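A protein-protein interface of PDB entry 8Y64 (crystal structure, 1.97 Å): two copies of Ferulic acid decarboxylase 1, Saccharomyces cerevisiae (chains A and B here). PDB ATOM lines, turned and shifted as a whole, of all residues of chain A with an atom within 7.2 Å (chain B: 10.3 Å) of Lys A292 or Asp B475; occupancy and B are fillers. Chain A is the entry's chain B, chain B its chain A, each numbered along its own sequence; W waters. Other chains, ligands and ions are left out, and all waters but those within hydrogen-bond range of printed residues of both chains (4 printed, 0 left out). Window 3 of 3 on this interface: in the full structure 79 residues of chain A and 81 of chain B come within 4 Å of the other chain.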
ATOM      1  N   VAL A 146     -37.859   7.235  -5.920  1.00  0.00           N
ATOM      2  CA  VAL A 146     -38.572   6.974  -7.162  1.00  0.00           C
ATOM      3  C   VAL A 146     -38.181   5.598  -7.688  1.00  0.00           C
ATOM      4  O   VAL A 146     -37.008   5.204  -7.646  1.00  0.00           O
ATOM      5  CB  VAL A 146     -38.270   8.088  -8.178  1.00  0.00           C
ATOM      6  CG1 VAL A 146     -38.676   7.671  -9.576  1.00  0.00           C
ATOM      7  CG2 VAL A 146     -38.971   9.389  -7.752  1.00  0.00           C
ATOM      8  N   SER A 147     -39.184   4.833  -8.138  1.00  0.00           N
ATOM      9  CA  SER A 147     -39.049   3.489  -8.702  1.00  0.00           C
ATOM     10  C   SER A 147     -38.535   2.433  -7.725  1.00  0.00           C
ATOM     11  O   SER A 147     -38.137   1.340  -8.167  1.00  0.00           O
ATOM     12  CB  SER A 147     -38.165   3.479  -9.963  1.00  0.00           C
ATOM     13  OG  SER A 147     -38.801   4.192 -11.012  1.00  0.00           O
ATOM     14  N   PRO A 282     -36.407  -3.149  -6.697  1.00  0.00           N
ATOM     15  CA  PRO A 282     -35.118  -2.503  -6.400  1.00  0.00           C
ATOM     16  C   PRO A 282     -35.254  -1.538  -5.242  1.00  0.00           C
ATOM     17  O   PRO A 282     -36.377  -1.188  -4.845  1.00  0.00           O
ATOM     18  CB  PRO A 282     -34.780  -1.768  -7.706  1.00  0.00           C
ATOM     19  CG  PRO A 282     -36.123  -1.473  -8.325  1.00  0.00           C
ATOM     20  CD  PRO A 282     -37.000  -2.652  -7.954  1.00  0.00           C
ATOM     21  N   TYR A 289     -27.826   4.817  -6.993  1.00  0.00           N
ATOM     22  CA  TYR A 289     -28.707   4.453  -8.101  1.00  0.00           C
ATOM     23  C   TYR A 289     -29.914   3.650  -7.640  1.00  0.00           C
ATOM     24  O   TYR A 289     -29.806   2.816  -6.740  1.00  0.00           O
ATOM     25  CB  TYR A 289     -27.988   3.570  -9.158  1.00  0.00           C
ATOM     26  CG  TYR A 289     -26.767   4.191  -9.775  1.00  0.00           C
ATOM     27  CD1 TYR A 289     -25.533   4.130  -9.133  1.00  0.00           C
ATOM     28  CD2 TYR A 289     -26.829   4.782 -11.037  1.00  0.00           C
ATOM     29  CE1 TYR A 289     -24.398   4.704  -9.700  1.00  0.00           C
ATOM     30  CE2 TYR A 289     -25.700   5.345 -11.617  1.00  0.00           C
ATOM     31  CZ  TYR A 289     -24.484   5.297 -10.942  1.00  0.00           C
ATOM     32  OH  TYR A 289     -23.360   5.855 -11.520  1.00  0.00           O
ATOM     33  N   VAL A 290     -31.054   3.870  -8.311  1.00  0.00           N
ATOM     34  CA  VAL A 290     -32.083   2.840  -8.461  1.00  0.00           C
ATOM     35  C   VAL A 290     -31.982   2.325  -9.894  1.00  0.00           C
ATOM     36  O   VAL A 290     -32.150   3.094 -10.855  1.00  0.00           O
ATOM     37  CB  VAL A 290     -33.503   3.366  -8.187  1.00  0.00           C
ATOM     38  CG1 VAL A 290     -34.518   2.209  -8.270  1.00  0.00           C
ATOM     39  CG2 VAL A 290     -33.599   4.119  -6.846  1.00  0.00           C
ATOM     40  N   PHE A 291     -31.721   1.032 -10.045  1.00  0.00           N
ATOM     41  CA  PHE A 291     -31.783   0.385 -11.349  1.00  0.00           C
ATOM     42  C   PHE A 291     -33.155  -0.265 -11.470  1.00  0.00           C
ATOM     43  O   PHE A 291     -33.507  -1.140 -10.669  1.00  0.00           O
ATOM     44  CB  PHE A 291     -30.643  -0.621 -11.526  1.00  0.00           C
ATOM     45  CG  PHE A 291     -29.287   0.034 -11.632  1.00  0.00           C
ATOM     46  CD1 PHE A 291     -28.989   0.879 -12.689  1.00  0.00           C
ATOM     47  CD2 PHE A 291     -28.328  -0.169 -10.661  1.00  0.00           C
ATOM     48  CE1 PHE A 291     -27.752   1.505 -12.773  1.00  0.00           C
ATOM     49  CE2 PHE A 291     -27.087   0.436 -10.744  1.00  0.00           C
ATOM     50  CZ  PHE A 291     -26.799   1.287 -11.799  1.00  0.00           C
ATOM     51  N   LYS A 292     -33.936   0.198 -12.436  1.00  0.00           N
ATOM     52  CA  LYS A 292     -35.351  -0.142 -12.481  1.00  0.00           C
ATOM     53  C   LYS A 292     -35.579  -1.608 -12.787  1.00  0.00           C
ATOM     54  O   LYS A 292     -34.753  -2.281 -13.414  1.00  0.00           O
ATOM     55  CB  LYS A 292     -36.100   0.707 -13.506  1.00  0.00           C
ATOM     56  CG  LYS A 292     -36.039   2.192 -13.260  1.00  0.00           C
ATOM     57  CD  LYS A 292     -36.523   2.960 -14.479  1.00  0.00           C
ATOM     58  CE  LYS A 292     -37.994   3.266 -14.431  1.00  0.00           C
ATOM     59  NZ  LYS A 292     -38.178   4.741 -14.549  1.00  0.00           N
ATOM     60  N   SER A 293     -36.714  -2.097 -12.283  1.00  0.00           N
ATOM     61  CA  SER A 293     -37.291  -3.400 -12.586  1.00  0.00           C
ATOM     62  C   SER A 293     -36.473  -4.546 -12.012  1.00  0.00           C
ATOM     63  O   SER A 293     -36.970  -5.677 -11.935  1.00  0.00           O
ATOM     64  CB  SER A 293     -37.474  -3.561 -14.099  1.00  0.00           C
ATOM     65  OG  SER A 293     -38.744  -3.062 -14.494  1.00  0.00           O
ATOM     66  N   GLN A 294     -35.234  -4.270 -11.590  1.00  0.00           N
ATOM     67  CA  GLN A 294     -34.432  -5.307 -10.951  1.00  0.00           C
ATOM     68  C   GLN A 294     -35.133  -5.798  -9.685  1.00  0.00           C
ATOM     69  O   GLN A 294     -35.141  -5.125  -8.651  1.00  0.00           O
ATOM     70  CB  GLN A 294     -32.986  -4.823 -10.694  1.00  0.00           C
ATOM     71  CG  GLN A 294     -32.751  -3.835  -9.532  1.00  0.00           C
ATOM     72  CD  GLN A 294     -31.390  -3.965  -8.845  1.00  0.00           C
ATOM     73  OE1 GLN A 294     -30.371  -3.469  -9.335  1.00  0.00           O
ATOM     74  NE2 GLN A 294     -31.385  -4.605  -7.675  1.00  0.00           N
ATOM     75  N   GLY A 295     -35.778  -6.961  -9.779  1.00  0.00           N
ATOM     76  CA  GLY A 295     -36.411  -7.579  -8.631  1.00  0.00           C
ATOM     77  C   GLY A 295     -35.887  -8.984  -8.430  1.00  0.00           C
ATOM     78  O   GLY A 295     -35.733  -9.736  -9.396  1.00  0.00           O
ATOM     79  N   GLN A 448     -24.236  -3.993 -13.682  1.00  0.00           N
ATOM     80  CA  GLN A 448     -24.586  -3.587 -15.042  1.00  0.00           C
ATOM     81  C   GLN A 448     -23.550  -4.057 -16.054  1.00  0.00           C
ATOM     82  O   GLN A 448     -23.250  -3.372 -17.032  1.00  0.00           O
ATOM     83  CB  GLN A 448     -24.781  -2.072 -15.111  1.00  0.00           C
ATOM     84  CG  GLN A 448     -25.780  -1.522 -14.044  1.00  0.00           C
ATOM     85  CD  GLN A 448     -27.096  -2.272 -14.006  1.00  0.00           C
ATOM     86  OE1 GLN A 448     -27.778  -2.393 -15.029  1.00  0.00           O
ATOM     87  NE2 GLN A 448     -27.472  -2.771 -12.826  1.00  0.00           N
ATOM     88  N   LEU B 369     -24.788  10.304 -25.962  1.00  0.00           N
ATOM     89  CA  LEU B 369     -25.103   8.881 -26.091  1.00  0.00           C
ATOM     90  C   LEU B 369     -25.796   8.570 -27.417  1.00  0.00           C
ATOM     91  O   LEU B 369     -25.585   7.493 -27.986  1.00  0.00           O
ATOM     92  CB  LEU B 369     -25.964   8.406 -24.912  1.00  0.00           C
ATOM     93  CG  LEU B 369     -25.262   8.339 -23.544  1.00  0.00           C
ATOM     94  CD1 LEU B 369     -26.138   7.630 -22.487  1.00  0.00           C
ATOM     95  CD2 LEU B 369     -23.870   7.675 -23.662  1.00  0.00           C
ATOM     96  N   GLN B 373     -24.244   5.782 -29.767  1.00  0.00           N
ATOM     97  CA  GLN B 373     -24.991   4.588 -30.134  1.00  0.00           C
ATOM     98  C   GLN B 373     -25.053   4.413 -31.651  1.00  0.00           C
ATOM     99  O   GLN B 373     -24.990   3.281 -32.145  1.00  0.00           O
ATOM    100  CB  GLN B 373     -26.379   4.662 -29.506  1.00  0.00           C
ATOM    101  CG  GLN B 373     -26.376   4.216 -28.025  1.00  0.00           C
ATOM    102  CD  GLN B 373     -27.494   4.850 -27.242  1.00  0.00           C
ATOM    103  OE1 GLN B 373     -28.548   5.114 -27.787  1.00  0.00           O
ATOM    104  NE2 GLN B 373     -27.291   5.050 -25.942  1.00  0.00           N
ATOM    105  N   ASP B 407     -23.804  11.577 -21.134  1.00  0.00           N
ATOM    106  CA  ASP B 407     -24.321  12.941 -21.138  1.00  0.00           C
ATOM    107  C   ASP B 407     -25.219  13.251 -19.932  1.00  0.00           C
ATOM    108  O   ASP B 407     -25.773  14.359 -19.863  1.00  0.00           O
ATOM    109  CB  ASP B 407     -25.097  13.235 -22.435  1.00  0.00           C
ATOM    110  CG  ASP B 407     -26.070  12.124 -22.817  1.00  0.00           C
ATOM    111  OD1 ASP B 407     -26.691  11.525 -21.915  1.00  0.00           O
ATOM    112  OD2 ASP B 407     -26.263  11.887 -24.031  1.00  0.00           O
ATOM    113  N   ASP B 408     -25.415  12.368 -18.957  1.00  0.00           N
ATOM    114  CA  ASP B 408     -26.143  12.747 -17.756  1.00  0.00           C
ATOM    115  C   ASP B 408     -25.241  13.316 -16.663  1.00  0.00           C
ATOM    116  O   ASP B 408     -25.744  13.689 -15.596  1.00  0.00           O
ATOM    117  CB  ASP B 408     -26.940  11.538 -17.241  1.00  0.00           C
ATOM    118  CG  ASP B 408     -26.055  10.461 -16.612  1.00  0.00           C
ATOM    119  OD1 ASP B 408     -26.499   9.847 -15.604  1.00  0.00           O
ATOM    120  OD2 ASP B 408     -24.903  10.271 -17.078  1.00  0.00           O
ATOM    121  N   ARG B 424     -18.902   3.819 -12.203  1.00  0.00           N
ATOM    122  CA  ARG B 424     -19.218   3.370 -13.557  1.00  0.00           C
ATOM    123  C   ARG B 424     -18.055   2.728 -14.297  1.00  0.00           C
ATOM    124  O   ARG B 424     -18.229   2.344 -15.448  1.00  0.00           O
ATOM    125  CB  ARG B 424     -19.766   4.533 -14.402  1.00  0.00           C
ATOM    126  CG  ARG B 424     -20.952   5.261 -13.731  1.00  0.00           C
ATOM    127  CD  ARG B 424     -21.728   6.133 -14.713  1.00  0.00           C
ATOM    128  NE  ARG B 424     -22.815   6.812 -14.018  1.00  0.00           N
ATOM    129  CZ  ARG B 424     -23.576   7.755 -14.552  1.00  0.00           C
ATOM    130  NH1 ARG B 424     -23.395   8.164 -15.802  1.00  0.00           N
ATOM    131  NH2 ARG B 424     -24.545   8.299 -13.815  1.00  0.00           N
ATOM    132  N   PHE B 466     -21.690   2.998 -19.100  1.00  0.00           N
ATOM    133  CA  PHE B 466     -22.212   1.644 -18.917  1.00  0.00           C
ATOM    134  C   PHE B 466     -22.316   0.932 -20.262  1.00  0.00           C
ATOM    135  O   PHE B 466     -22.616   1.548 -21.281  1.00  0.00           O
ATOM    136  CB  PHE B 466     -23.596   1.673 -18.266  1.00  0.00           C
ATOM    137  CG  PHE B 466     -23.596   2.085 -16.824  1.00  0.00           C
ATOM    138  CD1 PHE B 466     -22.935   1.322 -15.869  1.00  0.00           C
ATOM    139  CD2 PHE B 466     -24.278   3.225 -16.418  1.00  0.00           C
ATOM    140  CE1 PHE B 466     -22.945   1.699 -14.515  1.00  0.00           C
ATOM    141  CE2 PHE B 466     -24.296   3.608 -15.065  1.00  0.00           C
ATOM    142  CZ  PHE B 466     -23.635   2.834 -14.120  1.00  0.00           C
ATOM    143  N   GLN B 468     -24.563  -0.927 -21.577  1.00  0.00           N
ATOM    144  CA  GLN B 468     -25.856  -0.701 -22.220  1.00  0.00           C
ATOM    145  C   GLN B 468     -25.943   0.681 -22.862  1.00  0.00           C
ATOM    146  O   GLN B 468     -26.651   0.860 -23.863  1.00  0.00           O
ATOM    147  CB  GLN B 468     -26.984  -0.887 -21.202  1.00  0.00           C
ATOM    148  CG  GLN B 468     -28.396  -0.652 -21.752  1.00  0.00           C
ATOM    149  CD  GLN B 468     -29.476  -1.122 -20.788  1.00  0.00           C
ATOM    150  OE1 GLN B 468     -29.208  -1.901 -19.877  1.00  0.00           O
ATOM    151  NE2 GLN B 468     -30.683  -0.581 -20.936  1.00  0.00           N
ATOM    152  N   GLN B 469     -25.218   1.660 -22.326  1.00  0.00           N
ATOM    153  CA  GLN B 469     -25.256   3.001 -22.897  1.00  0.00           C
ATOM    154  C   GLN B 469     -24.558   3.074 -24.250  1.00  0.00           C
ATOM    155  O   GLN B 469     -24.743   4.058 -24.969  1.00  0.00           O
ATOM    156  CB  GLN B 469     -24.631   3.998 -21.921  1.00  0.00           C
ATOM    157  CG  GLN B 469     -25.512   4.254 -20.693  1.00  0.00           C
ATOM    158  CD  GLN B 469     -24.867   5.162 -19.660  1.00  0.00           C
ATOM    159  OE1 GLN B 469     -23.652   5.115 -19.432  1.00  0.00           O
ATOM    160  NE2 GLN B 469     -25.684   5.993 -19.018  1.00  0.00           N
ATOM    161  N   ARG B 472     -28.245   1.398 -26.277  1.00  0.00           N
ATOM    162  CA  ARG B 472     -29.627   1.859 -26.302  1.00  0.00           C
ATOM    163  C   ARG B 472     -29.887   2.661 -25.036  1.00  0.00           C
ATOM    164  O   ARG B 472     -28.989   2.865 -24.209  1.00  0.00           O
ATOM    165  CB  ARG B 472     -30.610   0.698 -26.382  1.00  0.00           C
ATOM    166  CG  ARG B 472     -30.559  -0.189 -25.151  1.00  0.00           C
ATOM    167  CD  ARG B 472     -30.934  -1.605 -25.455  1.00  0.00           C
ATOM    168  NE  ARG B 472     -31.118  -2.348 -24.217  1.00  0.00           N
ATOM    169  CZ  ARG B 472     -30.293  -3.289 -23.780  1.00  0.00           C
ATOM    170  NH1 ARG B 472     -29.184  -3.595 -24.438  1.00  0.00           N
ATOM    171  NH2 ARG B 472     -30.583  -3.933 -22.652  1.00  0.00           N
ATOM    172  N   SER B 473     -31.144   3.073 -24.870  1.00  0.00           N
ATOM    173  CA  SER B 473     -31.524   3.851 -23.697  1.00  0.00           C
ATOM    174  C   SER B 473     -31.312   3.040 -22.422  1.00  0.00           C
ATOM    175  O   SER B 473     -31.465   1.817 -22.394  1.00  0.00           O
ATOM    176  CB  SER B 473     -32.992   4.277 -23.775  1.00  0.00           C
ATOM    177  OG  SER B 473     -33.824   3.161 -24.058  1.00  0.00           O
ATOM    178  N   PHE B 474     -30.974   3.742 -21.349  1.00  0.00           N
ATOM    179  CA  PHE B 474     -30.771   3.108 -20.053  1.00  0.00           C
ATOM    180  C   PHE B 474     -31.289   4.086 -19.008  1.00  0.00           C
ATOM    181  O   PHE B 474     -30.648   5.102 -18.732  1.00  0.00           O
ATOM    182  CB  PHE B 474     -29.299   2.761 -19.855  1.00  0.00           C
ATOM    183  CG  PHE B 474     -29.002   2.023 -18.581  1.00  0.00           C
ATOM    184  CD1 PHE B 474     -29.989   1.316 -17.914  1.00  0.00           C
ATOM    185  CD2 PHE B 474     -27.715   2.020 -18.068  1.00  0.00           C
ATOM    186  CE1 PHE B 474     -29.701   0.637 -16.741  1.00  0.00           C
ATOM    187  CE2 PHE B 474     -27.416   1.341 -16.905  1.00  0.00           C
ATOM    188  CZ  PHE B 474     -28.413   0.647 -16.236  1.00  0.00           C
ATOM    189  N   ASP B 475     -32.461   3.786 -18.448  1.00  0.00           N
ATOM    190  CA  ASP B 475     -33.181   4.692 -17.549  1.00  0.00           C
ATOM    191  C   ASP B 475     -32.965   4.212 -16.121  1.00  0.00           C
ATOM    192  O   ASP B 475     -33.495   3.168 -15.727  1.00  0.00           O
ATOM    193  CB  ASP B 475     -34.668   4.728 -17.926  1.00  0.00           C
ATOM    194  CG  ASP B 475     -35.552   5.487 -16.915  1.00  0.00           C
ATOM    195  OD1 ASP B 475     -35.079   6.395 -16.203  1.00  0.00           O
ATOM    196  OD2 ASP B 475     -36.765   5.180 -16.864  1.00  0.00           O
ATOM    197  N   TYR B 476     -32.177   4.973 -15.351  1.00  0.00           N
ATOM    198  CA  TYR B 476     -31.938   4.712 -13.934  1.00  0.00           C
ATOM    199  C   TYR B 476     -32.179   5.992 -13.142  1.00  0.00           C
ATOM    200  O   TYR B 476     -32.196   7.098 -13.693  1.00  0.00           O
ATOM    201  CB  TYR B 476     -30.508   4.181 -13.669  1.00  0.00           C
ATOM    202  CG  TYR B 476     -29.400   4.968 -14.352  1.00  0.00           C
ATOM    203  CD1 TYR B 476     -28.905   6.161 -13.806  1.00  0.00           C
ATOM    204  CD2 TYR B 476     -28.854   4.518 -15.550  1.00  0.00           C
ATOM    205  CE1 TYR B 476     -27.887   6.884 -14.452  1.00  0.00           C
ATOM    206  CE2 TYR B 476     -27.847   5.217 -16.197  1.00  0.00           C
ATOM    207  CZ  TYR B 476     -27.375   6.399 -15.655  1.00  0.00           C
ATOM    208  OH  TYR B 476     -26.387   7.068 -16.335  1.00  0.00           O
ATOM    209  N   ILE B 477     -32.375   5.833 -11.834  1.00  0.00           N
ATOM    210  CA  ILE B 477     -32.625   6.960 -10.942  1.00  0.00           C
ATOM    211  C   ILE B 477     -31.308   7.385 -10.303  1.00  0.00           C
ATOM    212  O   ILE B 477     -30.550   6.544  -9.801  1.00  0.00           O
ATOM    213  CB  ILE B 477     -33.659   6.608  -9.859  1.00  0.00           C
ATOM    214  CG1 ILE B 477     -34.931   5.998 -10.487  1.00  0.00           C
ATOM    215  CG2 ILE B 477     -33.954   7.839  -8.987  1.00  0.00           C
ATOM    216  CD1 ILE B 477     -35.642   6.910 -11.485  1.00  0.00           C
ATOM    217  N   THR B 478     -31.035   8.683 -10.319  1.00  0.00           N
ATOM    218  CA  THR B 478     -29.887   9.244  -9.620  1.00  0.00           C
ATOM    219  C   THR B 478     -30.366   9.658  -8.233  1.00  0.00           C
ATOM    220  O   THR B 478     -31.216  10.539  -8.105  1.00  0.00           O
ATOM    221  CB  THR B 478     -29.303  10.418 -10.403  1.00  0.00           C
ATOM    222  OG1 THR B 478     -28.800   9.936 -11.659  1.00  0.00           O
ATOM    223  CG2 THR B 478     -28.196  11.095  -9.615  1.00  0.00           C
ATOM    224  N   CYS B 479     -29.848   9.000  -7.193  1.00  0.00           N
ATOM    225  CA  CYS B 479     -30.434   9.132  -5.852  1.00  0.00           C
ATOM    226  C   CYS B 479     -29.839  10.322  -5.092  1.00  0.00           C
ATOM    227  O   CYS B 479     -29.095  10.185  -4.119  1.00  0.00           O
ATOM    228  CB  CYS B 479     -30.266   7.837  -5.069  1.00  0.00           C
ATOM    229  SG  CYS B 479     -31.181   6.455  -5.815  1.00  0.00           S
ATOM    230  N   LYS B 483     -32.020  15.519  -8.492  1.00  0.00           N
ATOM    231  CA  LYS B 483     -32.270  14.588  -9.590  1.00  0.00           C
ATOM    232  C   LYS B 483     -33.139  13.403  -9.181  1.00  0.00           C
ATOM    233  O   LYS B 483     -33.649  12.690 -10.048  1.00  0.00           O
ATOM    234  CB  LYS B 483     -30.943  14.039 -10.143  1.00  0.00           C
ATOM    235  CG  LYS B 483     -29.923  15.068 -10.642  1.00  0.00           C
ATOM    236  CD  LYS B 483     -28.972  14.463 -11.708  1.00  0.00           C
ATOM    237  CE  LYS B 483     -27.499  14.892 -11.509  1.00  0.00           C
ATOM    238  NZ  LYS B 483     -26.441  13.968 -12.172  1.00  0.00           N
ATOM    239  N   GLY B 484     -33.283  13.135  -7.894  1.00  0.00           N
ATOM    240  CA  GLY B 484     -33.980  11.914  -7.546  1.00  0.00           C
ATOM    241  C   GLY B 484     -35.471  12.025  -7.404  1.00  0.00           C
ATOM    242  O   GLY B 484     -36.143  10.996  -7.322  1.00  0.00           O
HETATM  243  O   HOH W   1     -32.395   1.098 -14.555  1.00  0.00           O
HETATM  244  O   HOH W   2     -27.317  -2.354 -17.806  1.00  0.00           O
HETATM  245  O   HOH W   3     -35.514   9.005  -5.702  1.00  0.00           O
HETATM  246  O   HOH W   4     -24.812  -1.706 -18.904  1.00  0.00           O
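Of the printed residues of chain B, Phe A291 touches Phe B474 (3.6 Å) and Tyr B476 (3.8 Å).
Lys A292 touches one residue of chain B.
Gln A294 touches none of the printed residues of chain B.
Gln B468 touches none of the printed residues of chain A.
Printed residues of chain A within 4 Å of Phe B474: Phe A291 and Gln A448.
Asp B475 touches just one residue of chain A: Lys A292 (2.7 Å).
Of the printed residues of chain A, Ile B477 touches Val A146, Tyr A289 and Val A290.
Printed residues of chain A within 4 Å of Cys B479: Tyr A289 (3.6 Å) and Val A290 (3.5 Å).
Printed residues of chain A within 4 Å of Gly B484: Val A146 (3.3 Å).
The nearest residue of chain B that does not touch Lys A292 is Ile B477 (4.5 Å).
The nearest residue of chain A that does not touch Asp B475 is Val A290 (5.1 Å).
The nearest printed residue of chain A that does not touch Cys B479 is Val A146 (6.2 Å).
Water W1 lies within hydrogen-bond range of the backbone carbonyl oxygen of Asp B475 and the backbone NH of Lys A292.
Water W3 bridges the backbone carbonyl oxygen of Gly B484 (2.6 Å) and the backbone NH of Val A146 (2.9 Å).
Water W4 lies within hydrogen-bond range of the backbone NH of Gln B468 (2.8 Å) and the backbone carbonyl oxygen of Gln A448 (3.0 Å).
Water W2 bridges OE1 of Gln A448 (2.8 Å) and OE1 of Gln B468 (2.8 Å).
Of the 18 printed residues of chain B, 8 touch a printed residue of chain A.
Of the 11 printed residues of chain A, 6 touch a printed residue of chain B.
Among the printed residues, 15 pairs touch across the chains.
Among the printed residues, Asp or Glu carboxylates within 4 Å of a Lys or Arg side-chain nitrogen of the other chain: Lys A292 with Asp B475 (2.7 Å).
Among the printed residues, pairs that only touch across the chains: Val A146 with Ile B477 (3.6 Å), Val A146 with Gly B484 (3.3 Å), Tyr A289 with Phe B466 (3.995 Å), Tyr A289 with Tyr B476 (3.7 Å), Tyr A289 with Ile B477 (3.3 Å), Tyr A289 with Cys B479 (3.6 Å), Val A290 with Tyr B476 (3.4 Å), Phe A291 with Phe B474 (3.6 Å), Phe A291 with Tyr B476 (3.8 Å), Gln A448 with Phe B466 (3.9 Å) and Gln A448 with Phe B474 (3.3 Å).
The guanidinium group of Arg B424 is in hydrogen-bond range of the side-chain hydroxyl of Tyr A289 (2.7 Å).
The side-chain amino group (NZ) of Lys A292 is in salt-bridge range of the side-chain carboxylate (OD2) of Asp B475.
The backbone NH (N) of Ile B477 lies within hydrogen-bond range of the backbone carbonyl oxygen (O) of Val A290, 2.9 Å away.
The side-chain sulfur of Cys B479 sits close to the backbone NH of Val A290 (3.6 Å).
NH1 of Arg B424 lies within salt-bridge range of OD2 of Asp B408.
OD1 of Asp B408 lies within hydrogen-bond range of OH of Tyr B476.
OH of Tyr B476 is in hydrogen-bond range of NH1 of Arg B424, 3.2 Å away.
The side-chain amide oxygen of Gln B469 sits at hydrogen-bond distance from the backbone NH of Phe B466 (2.9 Å).
The side-chain amide nitrogen of Gln B469 lies within hydrogen-bond range of the side-chain hydroxyl of Tyr B476 (3.0 Å).
The backbone carbonyl oxygen of Thr B478 lies close to the backbone NH of Gly B484 (3.3 Å).
No position is printed for both chains.
Of the 15 pairs that touch across the chains among the printed residues, none has its exchanged pair printed and touching as well.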
